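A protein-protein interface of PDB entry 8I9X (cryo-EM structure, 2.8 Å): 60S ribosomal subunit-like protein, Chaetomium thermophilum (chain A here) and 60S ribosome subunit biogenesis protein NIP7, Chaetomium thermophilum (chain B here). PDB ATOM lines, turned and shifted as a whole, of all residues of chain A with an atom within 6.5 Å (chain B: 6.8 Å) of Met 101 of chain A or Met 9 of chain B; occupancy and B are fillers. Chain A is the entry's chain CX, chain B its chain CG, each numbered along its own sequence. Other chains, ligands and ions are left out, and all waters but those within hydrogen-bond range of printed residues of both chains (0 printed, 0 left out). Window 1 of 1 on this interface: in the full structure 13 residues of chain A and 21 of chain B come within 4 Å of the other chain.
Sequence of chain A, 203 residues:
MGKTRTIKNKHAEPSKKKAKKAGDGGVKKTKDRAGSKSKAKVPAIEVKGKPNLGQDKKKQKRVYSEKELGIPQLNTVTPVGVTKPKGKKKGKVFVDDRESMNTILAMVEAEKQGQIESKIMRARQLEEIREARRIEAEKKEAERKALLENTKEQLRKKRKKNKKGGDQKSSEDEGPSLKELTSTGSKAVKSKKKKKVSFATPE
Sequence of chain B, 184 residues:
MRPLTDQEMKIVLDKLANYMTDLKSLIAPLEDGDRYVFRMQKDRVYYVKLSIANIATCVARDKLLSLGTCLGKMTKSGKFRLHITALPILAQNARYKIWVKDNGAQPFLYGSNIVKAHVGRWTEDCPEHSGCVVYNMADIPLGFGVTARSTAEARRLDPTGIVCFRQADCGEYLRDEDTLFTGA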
ATOM      1  N   VAL A  95     -11.365 -26.747  20.950  1.00  0.00           N
ATOM      2  CA  VAL A  95     -10.684 -27.771  21.727  1.00  0.00           C
ATOM      3  C   VAL A  95     -11.686 -28.300  22.740  1.00  0.00           C
ATOM      4  O   VAL A  95     -11.849 -27.730  23.826  1.00  0.00           O
ATOM      5  CB  VAL A  95      -9.422 -27.236  22.415  1.00  0.00           C
ATOM      6  CG1 VAL A  95      -8.806 -28.306  23.298  1.00  0.00           C
ATOM      7  CG2 VAL A  95      -8.421 -26.779  21.373  1.00  0.00           C
ATOM      8  N   ASP A  96     -12.373 -29.379  22.375  1.00  0.00           N
ATOM      9  CA  ASP A  96     -13.289 -30.060  23.272  1.00  0.00           C
ATOM     10  C   ASP A  96     -12.964 -31.535  23.430  1.00  0.00           C
ATOM     11  O   ASP A  96     -13.709 -32.242  24.118  1.00  0.00           O
ATOM     12  CB  ASP A  96     -14.738 -29.911  22.780  1.00  0.00           C
ATOM     13  CG  ASP A  96     -15.750 -30.024  23.902  1.00  0.00           C
ATOM     14  OD1 ASP A  96     -15.428 -29.618  25.037  1.00  0.00           O
ATOM     15  OD2 ASP A  96     -16.870 -30.516  23.646  1.00  0.00           O
ATOM     16  N   ASP A  97     -11.886 -32.018  22.822  1.00  0.00           N
ATOM     17  CA  ASP A  97     -11.503 -33.414  22.943  1.00  0.00           C
ATOM     18  C   ASP A  97     -10.614 -33.622  24.161  1.00  0.00           C
ATOM     19  O   ASP A  97      -9.801 -32.763  24.519  1.00  0.00           O
ATOM     20  CB  ASP A  97     -10.783 -33.886  21.680  1.00  0.00           C
ATOM     21  CG  ASP A  97     -11.670 -33.843  20.455  1.00  0.00           C
ATOM     22  OD1 ASP A  97     -12.707 -33.148  20.495  1.00  0.00           O
ATOM     23  OD2 ASP A  97     -11.335 -34.507  19.453  1.00  0.00           O
ATOM     24  N   ARG A  98     -10.777 -34.786  24.789  1.00  0.00           N
ATOM     25  CA  ARG A  98     -10.022 -35.105  25.992  1.00  0.00           C
ATOM     26  C   ARG A  98      -8.529 -35.158  25.688  1.00  0.00           C
ATOM     27  O   ARG A  98      -7.711 -34.694  26.490  1.00  0.00           O
ATOM     28  CB  ARG A  98     -10.552 -36.430  26.551  1.00  0.00           C
ATOM     29  CG  ARG A  98     -10.074 -36.889  27.922  1.00  0.00           C
ATOM     30  CD  ARG A  98      -8.881 -37.812  27.888  1.00  0.00           C
ATOM     31  NE  ARG A  98      -8.583 -38.318  29.223  1.00  0.00           N
ATOM     32  CZ  ARG A  98      -7.873 -37.670  30.136  1.00  0.00           C
ATOM     33  NH1 ARG A  98      -7.449 -36.436  29.934  1.00  0.00           N
ATOM     34  NH2 ARG A  98      -7.608 -38.268  31.294  1.00  0.00           N
ATOM     35  N   GLU A  99      -8.163 -35.644  24.500  1.00  0.00           N
ATOM     36  CA  GLU A  99      -6.763 -35.722  24.089  1.00  0.00           C
ATOM     37  C   GLU A  99      -6.161 -34.347  23.814  1.00  0.00           C
ATOM     38  O   GLU A  99      -5.006 -34.086  24.175  1.00  0.00           O
ATOM     39  CB  GLU A  99      -6.643 -36.609  22.851  1.00  0.00           C
ATOM     40  CG  GLU A  99      -6.966 -38.073  23.097  1.00  0.00           C
ATOM     41  CD  GLU A  99      -8.453 -38.359  23.067  1.00  0.00           C
ATOM     42  OE1 GLU A  99      -9.232 -37.423  22.794  1.00  0.00           O
ATOM     43  OE2 GLU A  99      -8.842 -39.521  23.307  1.00  0.00           O
ATOM     44  N   SER A 100      -6.907 -33.467  23.143  1.00  0.00           N
ATOM     45  CA  SER A 100      -6.415 -32.112  22.916  1.00  0.00           C
ATOM     46  C   SER A 100      -6.245 -31.359  24.228  1.00  0.00           C
ATOM     47  O   SER A 100      -5.253 -30.633  24.413  1.00  0.00           O
ATOM     48  CB  SER A 100      -7.363 -31.361  21.984  1.00  0.00           C
ATOM     49  OG  SER A 100      -7.397 -31.964  20.702  1.00  0.00           O
ATOM     50  N   MET A 101      -7.193 -31.521  25.148  1.00  0.00           N
ATOM     51  CA  MET A 101      -7.005 -30.953  26.474  1.00  0.00           C
ATOM     52  C   MET A 101      -5.770 -31.543  27.145  1.00  0.00           C
ATOM     53  O   MET A 101      -5.026 -30.818  27.810  1.00  0.00           O
ATOM     54  CB  MET A 101      -8.254 -31.177  27.326  1.00  0.00           C
ATOM     55  CG  MET A 101      -9.290 -30.075  27.171  1.00  0.00           C
ATOM     56  SD  MET A 101     -10.547 -30.083  28.460  1.00  0.00           S
ATOM     57  CE  MET A 101     -11.566 -31.453  27.930  1.00  0.00           C
ATOM     58  N   ASN A 102      -5.523 -32.843  26.957  1.00  0.00           N
ATOM     59  CA  ASN A 102      -4.320 -33.456  27.511  1.00  0.00           C
ATOM     60  C   ASN A 102      -3.046 -32.822  26.977  1.00  0.00           C
ATOM     61  O   ASN A 102      -2.126 -32.556  27.753  1.00  0.00           O
ATOM     62  CB  ASN A 102      -4.291 -34.956  27.224  1.00  0.00           C
ATOM     63  CG  ASN A 102      -5.097 -35.750  28.213  1.00  0.00           C
ATOM     64  OD1 ASN A 102      -6.041 -36.445  27.849  1.00  0.00           O
ATOM     65  ND2 ASN A 102      -4.720 -35.660  29.482  1.00  0.00           N
ATOM     66  N   THR A 103      -2.953 -32.595  25.667  1.00  0.00           N
ATOM     67  CA  THR A 103      -1.700 -32.065  25.131  1.00  0.00           C
ATOM     68  C   THR A 103      -1.490 -30.612  25.552  1.00  0.00           C
ATOM     69  O   THR A 103      -0.372 -30.215  25.917  1.00  0.00           O
ATOM     70  CB  THR A 103      -1.643 -32.212  23.607  1.00  0.00           C
ATOM     71  OG1 THR A 103      -0.434 -31.620  23.117  1.00  0.00           O
ATOM     72  CG2 THR A 103      -2.808 -31.538  22.947  1.00  0.00           C
ATOM     73  N   ILE A 104      -2.556 -29.805  25.531  1.00  0.00           N
ATOM     74  CA  ILE A 104      -2.427 -28.425  25.994  1.00  0.00           C
ATOM     75  C   ILE A 104      -2.028 -28.401  27.463  1.00  0.00           C
ATOM     76  O   ILE A 104      -1.159 -27.621  27.879  1.00  0.00           O
ATOM     77  CB  ILE A 104      -3.731 -27.649  25.743  1.00  0.00           C
ATOM     78  CG1 ILE A 104      -3.974 -27.485  24.243  1.00  0.00           C
ATOM     79  CG2 ILE A 104      -3.686 -26.292  26.421  1.00  0.00           C
ATOM     80  CD1 ILE A 104      -5.349 -26.968  23.904  1.00  0.00           C
ATOM     81  N   LEU A 105      -2.642 -29.272  28.265  1.00  0.00           N
ATOM     82  CA  LEU A 105      -2.328 -29.360  29.684  1.00  0.00           C
ATOM     83  C   LEU A 105      -0.887 -29.792  29.910  1.00  0.00           C
ATOM     84  O   LEU A 105      -0.212 -29.279  30.809  1.00  0.00           O
ATOM     85  CB  LEU A 105      -3.299 -30.339  30.336  1.00  0.00           C
ATOM     86  CG  LEU A 105      -3.484 -30.425  31.840  1.00  0.00           C
ATOM     87  CD1 LEU A 105      -4.909 -30.851  32.079  1.00  0.00           C
ATOM     88  CD2 LEU A 105      -2.525 -31.427  32.443  1.00  0.00           C
ATOM     89  N   ALA A 106      -0.407 -30.752  29.121  1.00  0.00           N
ATOM     90  CA  ALA A 106       0.968 -31.213  29.261  1.00  0.00           C
ATOM     91  C   ALA A 106       1.950 -30.091  28.971  1.00  0.00           C
ATOM     92  O   ALA A 106       2.910 -29.890  29.724  1.00  0.00           O
ATOM     93  CB  ALA A 106       1.221 -32.403  28.338  1.00  0.00           C
ATOM     94  N   VAL A 108       1.328 -26.862  29.247  1.00  0.00           N
ATOM     95  CA  VAL A 108       1.184 -25.859  30.299  1.00  0.00           C
ATOM     96  C   VAL A 108       1.951 -26.285  31.545  1.00  0.00           C
ATOM     97  O   VAL A 108       2.702 -25.498  32.132  1.00  0.00           O
ATOM     98  CB  VAL A 108      -0.305 -25.621  30.607  1.00  0.00           C
ATOM     99  CG1 VAL A 108      -0.474 -24.964  31.968  1.00  0.00           C
ATOM    100  CG2 VAL A 108      -0.943 -24.782  29.516  1.00  0.00           C
ATOM    101  N   PRO B   3     -17.743 -24.325  22.871  1.00  0.00           N
ATOM    102  CA  PRO B   3     -16.504 -24.775  23.511  1.00  0.00           C
ATOM    103  C   PRO B   3     -15.415 -23.719  23.401  1.00  0.00           C
ATOM    104  O   PRO B   3     -15.497 -22.767  22.623  1.00  0.00           O
ATOM    105  CB  PRO B   3     -16.139 -26.043  22.733  1.00  0.00           C
ATOM    106  CG  PRO B   3     -17.417 -26.478  22.090  1.00  0.00           C
ATOM    107  CD  PRO B   3     -18.134 -25.210  21.761  1.00  0.00           C
ATOM    108  N   LEU B   4     -14.374 -23.895  24.209  1.00  0.00           N
ATOM    109  CA  LEU B   4     -13.230 -23.002  24.155  1.00  0.00           C
ATOM    110  C   LEU B   4     -12.322 -23.360  22.981  1.00  0.00           C
ATOM    111  O   LEU B   4     -12.234 -24.515  22.556  1.00  0.00           O
ATOM    112  CB  LEU B   4     -12.438 -23.061  25.462  1.00  0.00           C
ATOM    113  CG  LEU B   4     -13.051 -22.368  26.679  1.00  0.00           C
ATOM    114  CD1 LEU B   4     -12.083 -22.401  27.846  1.00  0.00           C
ATOM    115  CD2 LEU B   4     -13.433 -20.941  26.344  1.00  0.00           C
ATOM    116  N   THR B   5     -11.644 -22.346  22.454  1.00  0.00           N
ATOM    117  CA  THR B   5     -10.649 -22.546  21.414  1.00  0.00           C
ATOM    118  C   THR B   5      -9.300 -22.887  22.043  1.00  0.00           C
ATOM    119  O   THR B   5      -9.163 -22.987  23.262  1.00  0.00           O
ATOM    120  CB  THR B   5     -10.531 -21.307  20.530  1.00  0.00           C
ATOM    121  OG1 THR B   5     -10.096 -20.192  21.318  1.00  0.00           O
ATOM    122  CG2 THR B   5     -11.872 -20.979  19.896  1.00  0.00           C
ATOM    123  N   ASP B   6      -8.292 -23.077  21.190  1.00  0.00           N
ATOM    124  CA  ASP B   6      -6.985 -23.507  21.682  1.00  0.00           C
ATOM    125  C   ASP B   6      -6.300 -22.427  22.520  1.00  0.00           C
ATOM    126  O   ASP B   6      -5.787 -22.715  23.608  1.00  0.00           O
ATOM    127  CB  ASP B   6      -6.111 -23.970  20.511  1.00  0.00           C
ATOM    128  CG  ASP B   6      -5.830 -22.871  19.516  1.00  0.00           C
ATOM    129  OD1 ASP B   6      -6.351 -21.757  19.706  1.00  0.00           O
ATOM    130  OD2 ASP B   6      -5.088 -23.120  18.542  1.00  0.00           O
ATOM    131  N   GLN B   7      -6.285 -21.176  22.046  1.00  0.00           N
ATOM    132  CA  GLN B   7      -5.680 -20.110  22.846  1.00  0.00           C
ATOM    133  C   GLN B   7      -6.442 -19.888  24.147  1.00  0.00           C
ATOM    134  O   GLN B   7      -5.835 -19.679  25.206  1.00  0.00           O
ATOM    135  CB  GLN B   7      -5.599 -18.796  22.064  1.00  0.00           C
ATOM    136  CG  GLN B   7      -4.423 -18.664  21.100  1.00  0.00           C
ATOM    137  CD  GLN B   7      -4.595 -19.449  19.821  1.00  0.00           C
ATOM    138  OE1 GLN B   7      -5.597 -19.301  19.122  1.00  0.00           O
ATOM    139  NE2 GLN B   7      -3.617 -20.288  19.503  1.00  0.00           N
ATOM    140  N   GLU B   8      -7.775 -19.911  24.084  1.00  0.00           N
ATOM    141  CA  GLU B   8      -8.577 -19.718  25.286  1.00  0.00           C
ATOM    142  C   GLU B   8      -8.319 -20.824  26.299  1.00  0.00           C
ATOM    143  O   GLU B   8      -8.173 -20.557  27.499  1.00  0.00           O
ATOM    144  CB  GLU B   8     -10.058 -19.667  24.916  1.00  0.00           C
ATOM    145  CG  GLU B   8     -10.538 -18.308  24.444  1.00  0.00           C
ATOM    146  CD  GLU B   8     -12.027 -18.282  24.170  1.00  0.00           C
ATOM    147  OE1 GLU B   8     -12.524 -19.206  23.492  1.00  0.00           O
ATOM    148  OE2 GLU B   8     -12.703 -17.340  24.631  1.00  0.00           O
ATOM    149  N   MET B   9      -8.253 -22.071  25.828  1.00  0.00           N
ATOM    150  CA  MET B   9      -7.943 -23.190  26.707  1.00  0.00           C
ATOM    151  C   MET B   9      -6.555 -23.048  27.308  1.00  0.00           C
ATOM    152  O   MET B   9      -6.369 -23.318  28.500  1.00  0.00           O
ATOM    153  CB  MET B   9      -8.060 -24.505  25.939  1.00  0.00           C
ATOM    154  CG  MET B   9      -7.875 -25.748  26.787  1.00  0.00           C
ATOM    155  SD  MET B   9      -9.150 -25.925  28.045  1.00  0.00           S
ATOM    156  CE  MET B   9     -10.557 -26.381  27.036  1.00  0.00           C
ATOM    157  N   LYS B  10      -5.581 -22.611  26.510  1.00  0.00           N
ATOM    158  CA  LYS B  10      -4.228 -22.425  27.017  1.00  0.00           C
ATOM    159  C   LYS B  10      -4.199 -21.383  28.130  1.00  0.00           C
ATOM    160  O   LYS B  10      -3.565 -21.587  29.169  1.00  0.00           O
ATOM    161  CB  LYS B  10      -3.293 -22.031  25.873  1.00  0.00           C
ATOM    162  CG  LYS B  10      -1.841 -21.870  26.287  1.00  0.00           C
ATOM    163  CD  LYS B  10      -0.955 -21.591  25.087  1.00  0.00           C
ATOM    164  CE  LYS B  10       0.469 -21.282  25.513  1.00  0.00           C
ATOM    165  NZ  LYS B  10       1.130 -22.461  26.136  1.00  0.00           N
ATOM    166  N   ILE B  11      -4.903 -20.266  27.939  1.00  0.00           N
ATOM    167  CA  ILE B  11      -4.904 -19.206  28.949  1.00  0.00           C
ATOM    168  C   ILE B  11      -5.609 -19.665  30.224  1.00  0.00           C
ATOM    169  O   ILE B  11      -5.115 -19.456  31.347  1.00  0.00           O
ATOM    170  CB  ILE B  11      -5.548 -17.929  28.377  1.00  0.00           C
ATOM    171  CG1 ILE B  11      -4.742 -17.424  27.181  1.00  0.00           C
ATOM    172  CG2 ILE B  11      -5.645 -16.854  29.445  1.00  0.00           C
ATOM    173  CD1 ILE B  11      -5.467 -16.397  26.352  1.00  0.00           C
ATOM    174  N   VAL B  12      -6.780 -20.289  30.069  1.00  0.00           N
ATOM    175  CA  VAL B  12      -7.535 -20.749  31.228  1.00  0.00           C
ATOM    176  C   VAL B  12      -6.725 -21.768  32.018  1.00  0.00           C
ATOM    177  O   VAL B  12      -6.640 -21.695  33.250  1.00  0.00           O
ATOM    178  CB  VAL B  12      -8.896 -21.314  30.784  1.00  0.00           C
ATOM    179  CG1 VAL B  12      -9.566 -22.054  31.922  1.00  0.00           C
ATOM    180  CG2 VAL B  12      -9.791 -20.197  30.279  1.00  0.00           C
ATOM    181  N   LEU B  13      -6.098 -22.721  31.325  1.00  0.00           N
ATOM    182  CA  LEU B  13      -5.268 -23.704  32.000  1.00  0.00           C
ATOM    183  C   LEU B  13      -3.997 -23.103  32.576  1.00  0.00           C
ATOM    184  O   LEU B  13      -3.496 -23.617  33.575  1.00  0.00           O
ATOM    185  CB  LEU B  13      -4.923 -24.846  31.045  1.00  0.00           C
ATOM    186  CG  LEU B  13      -6.103 -25.758  30.714  1.00  0.00           C
ATOM    187  CD1 LEU B  13      -5.728 -26.759  29.636  1.00  0.00           C
ATOM    188  CD2 LEU B  13      -6.606 -26.464  31.961  1.00  0.00           C
ATOM    189  N   ASP B  14      -3.468 -22.028  31.989  1.00  0.00           N
ATOM    190  CA  ASP B  14      -2.339 -21.343  32.609  1.00  0.00           C
ATOM    191  C   ASP B  14      -2.720 -20.779  33.970  1.00  0.00           C
ATOM    192  O   ASP B  14      -1.997 -20.977  34.953  1.00  0.00           O
ATOM    193  CB  ASP B  14      -1.823 -20.232  31.696  1.00  0.00           C
ATOM    194  CG  ASP B  14      -1.005 -20.762  30.536  1.00  0.00           C
ATOM    195  OD1 ASP B  14      -0.351 -21.812  30.698  1.00  0.00           O
ATOM    196  OD2 ASP B  14      -1.015 -20.126  29.460  1.00  0.00           O
ATOM    197  N   LEU B  16      -5.276 -21.771  35.843  1.00  0.00           N
ATOM    198  CA  LEU B  16      -5.633 -22.893  36.693  1.00  0.00           C
ATOM    199  C   LEU B  16      -4.415 -23.652  37.197  1.00  0.00           C
ATOM    200  O   LEU B  16      -4.445 -24.145  38.324  1.00  0.00           O
ATOM    201  CB  LEU B  16      -6.565 -23.837  35.935  1.00  0.00           C
ATOM    202  CG  LEU B  16      -8.001 -23.343  35.761  1.00  0.00           C
ATOM    203  CD1 LEU B  16      -8.729 -24.186  34.729  1.00  0.00           C
ATOM    204  CD2 LEU B  16      -8.751 -23.326  37.073  1.00  0.00           C
ATOM    205  N   LYS B  24      -5.036 -32.947  35.048  1.00  0.00           N
ATOM    206  CA  LYS B  24      -5.603 -34.177  34.520  1.00  0.00           C
ATOM    207  C   LYS B  24      -6.683 -34.726  35.439  1.00  0.00           C
ATOM    208  O   LYS B  24      -7.575 -35.436  34.970  1.00  0.00           O
ATOM    209  CB  LYS B  24      -4.514 -35.228  34.305  1.00  0.00           C
ATOM    210  CG  LYS B  24      -3.506 -34.879  33.224  1.00  0.00           C
ATOM    211  CD  LYS B  24      -2.485 -35.991  33.052  1.00  0.00           C
ATOM    212  CE  LYS B  24      -1.366 -35.581  32.110  1.00  0.00           C
ATOM    213  NZ  LYS B  24      -1.842 -35.449  30.705  1.00  0.00           N
ATOM    214  N   ILE B  27      -9.705 -32.917  34.108  1.00  0.00           N
ATOM    215  CA  ILE B  27     -10.201 -33.341  32.804  1.00  0.00           C
ATOM    216  C   ILE B  27     -10.344 -34.862  32.712  1.00  0.00           C
ATOM    217  O   ILE B  27     -10.586 -35.391  31.637  1.00  0.00           O
ATOM    218  CB  ILE B  27      -9.325 -32.813  31.652  1.00  0.00           C
ATOM    219  CG1 ILE B  27      -7.907 -33.369  31.747  1.00  0.00           C
ATOM    220  CG2 ILE B  27      -9.307 -31.295  31.658  1.00  0.00           C
ATOM    221  CD1 ILE B  27      -7.078 -33.079  30.519  1.00  0.00           C
ATOM    222  N   ARG B  35     -17.240 -36.796  31.574  1.00  0.00           N
ATOM    223  CA  ARG B  35     -16.071 -35.990  31.884  1.00  0.00           C
ATOM    224  C   ARG B  35     -16.486 -34.536  32.024  1.00  0.00           C
ATOM    225  O   ARG B  35     -17.541 -34.126  31.534  1.00  0.00           O
ATOM    226  CB  ARG B  35     -14.996 -36.122  30.801  1.00  0.00           C
ATOM    227  CG  ARG B  35     -15.521 -35.884  29.402  1.00  0.00           C
ATOM    228  CD  ARG B  35     -14.553 -36.380  28.352  1.00  0.00           C
ATOM    229  NE  ARG B  35     -14.943 -35.957  27.014  1.00  0.00           N
ATOM    230  CZ  ARG B  35     -14.679 -34.765  26.498  1.00  0.00           C
ATOM    231  NH1 ARG B  35     -14.009 -33.851  27.179  1.00  0.00           N
ATOM    232  NH2 ARG B  35     -15.096 -34.484  25.267  1.00  0.00           N
ATOM    233  N   TYR B  36     -15.643 -33.759  32.695  1.00  0.00           N
ATOM    234  CA  TYR B  36     -15.873 -32.331  32.821  1.00  0.00           C
ATOM    235  C   TYR B  36     -15.283 -31.612  31.616  1.00  0.00           C
ATOM    236  O   TYR B  36     -14.132 -31.852  31.243  1.00  0.00           O
ATOM    237  CB  TYR B  36     -15.251 -31.796  34.108  1.00  0.00           C
ATOM    238  CG  TYR B  36     -16.156 -31.865  35.311  1.00  0.00           C
ATOM    239  CD1 TYR B  36     -16.837 -30.745  35.757  1.00  0.00           C
ATOM    240  CD2 TYR B  36     -16.300 -33.043  36.023  1.00  0.00           C
ATOM    241  CE1 TYR B  36     -17.655 -30.802  36.865  1.00  0.00           C
ATOM    242  CE2 TYR B  36     -17.110 -33.111  37.133  1.00  0.00           C
ATOM    243  CZ  TYR B  36     -17.788 -31.989  37.549  1.00  0.00           C
ATOM    244  OH  TYR B  36     -18.602 -32.050  38.657  1.00  0.00           O
ATOM    245  N   VAL B  37     -16.073 -30.733  31.007  1.00  0.00           N
ATOM    246  CA  VAL B  37     -15.621 -29.977  29.847  1.00  0.00           C
ATOM    247  C   VAL B  37     -15.704 -28.489  30.149  1.00  0.00           C
ATOM    248  O   VAL B  37     -16.202 -28.083  31.204  1.00  0.00           O
ATOM    249  CB  VAL B  37     -16.437 -30.336  28.593  1.00  0.00           C
ATOM    250  CG1 VAL B  37     -16.493 -31.841  28.414  1.00  0.00           C
ATOM    251  CG2 VAL B  37     -17.836 -29.759  28.692  1.00  0.00           C
ATOM    252  N   PHE B  38     -15.216 -27.667  29.225  1.00  0.00           N
ATOM    253  CA  PHE B  38     -15.191 -26.219  29.380  1.00  0.00           C
ATOM    254  C   PHE B  38     -16.147 -25.609  28.367  1.00  0.00           C
ATOM    255  O   PHE B  38     -16.188 -26.042  27.211  1.00  0.00           O
ATOM    256  CB  PHE B  38     -13.780 -25.666  29.178  1.00  0.00           C
ATOM    257  CG  PHE B  38     -12.859 -25.917  30.333  1.00  0.00           C
ATOM    258  CD1 PHE B  38     -12.665 -24.952  31.303  1.00  0.00           C
ATOM    259  CD2 PHE B  38     -12.174 -27.114  30.442  1.00  0.00           C
ATOM    260  CE1 PHE B  38     -11.813 -25.182  32.361  1.00  0.00           C
ATOM    261  CE2 PHE B  38     -11.323 -27.346  31.500  1.00  0.00           C
ATOM    262  CZ  PHE B  38     -11.141 -26.378  32.460  1.00  0.00           C
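N of Val 95 of chain A lies within hydrogen-bond range of O of Leu 4 of chain B, 2.9 Å away.
NH2 of Arg 35 of chain B is in hydrogen-bond range of O of Asp 96 of chain A.
The side-chain amide nitrogen (ND2) of Asn 102 of chain A sits close to the side-chain amino group (NZ) of Lys 24 of chain B, 3.1 Å away.
The guanidinium group (NH1) of Arg 98 of chain A sits at hydrogen-bond distance from the side-chain amide oxygen (OD1) of Asn 102 of chain A (2.5 Å).
The side-chain carboxylate (OD1) of Asp 6 of chain B lies close to the side-chain amide oxygen (OE1) of Gln 7 of chain B (2.6 Å).
Among the printed residues, pairs that only touch across the chains: Val 108 of chain A with Asp 14 of chain B, Arg 98 of chain A with Ile 27 of chain B, Leu 105 of chain A with Ile 27 of chain B, Met 101 of chain A with Arg 35 of chain B, Val 95 of chain A with Asp 6 of chain B, Leu 105 of chain A with Lys 24 of chain B, Met 101 of chain A with Ile 27 of chain B, Asn 102 of chain A with Ile 27 of chain B, Val 108 of chain A with Leu 13 of chain B, Val 95 of chain A with Met 9 of chain B, Asp 96 of chain A with Val 37 of chain B, Ile 104 of chain A with Leu 13 of chain B, Met 101 of chain A with Met 9 of chain B, Met 101 of chain A with Phe 38 of chain B and Ile 104 of chain A with Lys 10 of chain B.
Of chain B, only Met 9 (3.9 Å), Ile 27 (3.6 Å), Arg 35 (3.5 Å) and Phe 38 (3.9 Å) come within 4 Å of Met 101 of chain A.
Printed residues of chain A within 4 Å of Phe 38 of chain B: Met 101 (3.9 Å).
Printed residues of chain A within 4 Å of Leu 13 of chain B: Ile 104 (3.8 Å) and Val 108 (3.7 Å).
The nearest residue of chain B that does not touch Met 101 of chain A is Tyr 36 of chain B (4.2 Å).
The nearest printed residue of chain A that does not touch Leu 4 of chain B is Asp 96 of chain A (4.9 Å).
Printed residues of chain B that touch a printed residue of chain A: Leu 4, Asp 6, Met 9, Lys 10, Leu 13, Asp 14, Lys 24, Ile 27, Arg 35, Val 37 and Phe 38.
Of the 13 printed residues of chain A, 8 touch a printed residue of chain B.
Printed residues of chain A that touch a printed residue of chain B: Val 95, Asp 96, Arg 98, Met 101, Asn 102, Ile 104, Leu 105 and Val 108.
Hydrophobic or aromatic side chains of chain A that line the printed part of chain B: Val 95, Met 101, Ile 104, Leu 105 and Val 108.
Along chain A the printed residues that touch a printed residue of chain B span positions 95 to 108.
Among the printed residues, 18 pairs touch across the chains.
Among the printed residues, no Asp or Glu carboxylate lies within 4 Å of a Lys or Arg side-chain nitrogen of the other chain.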
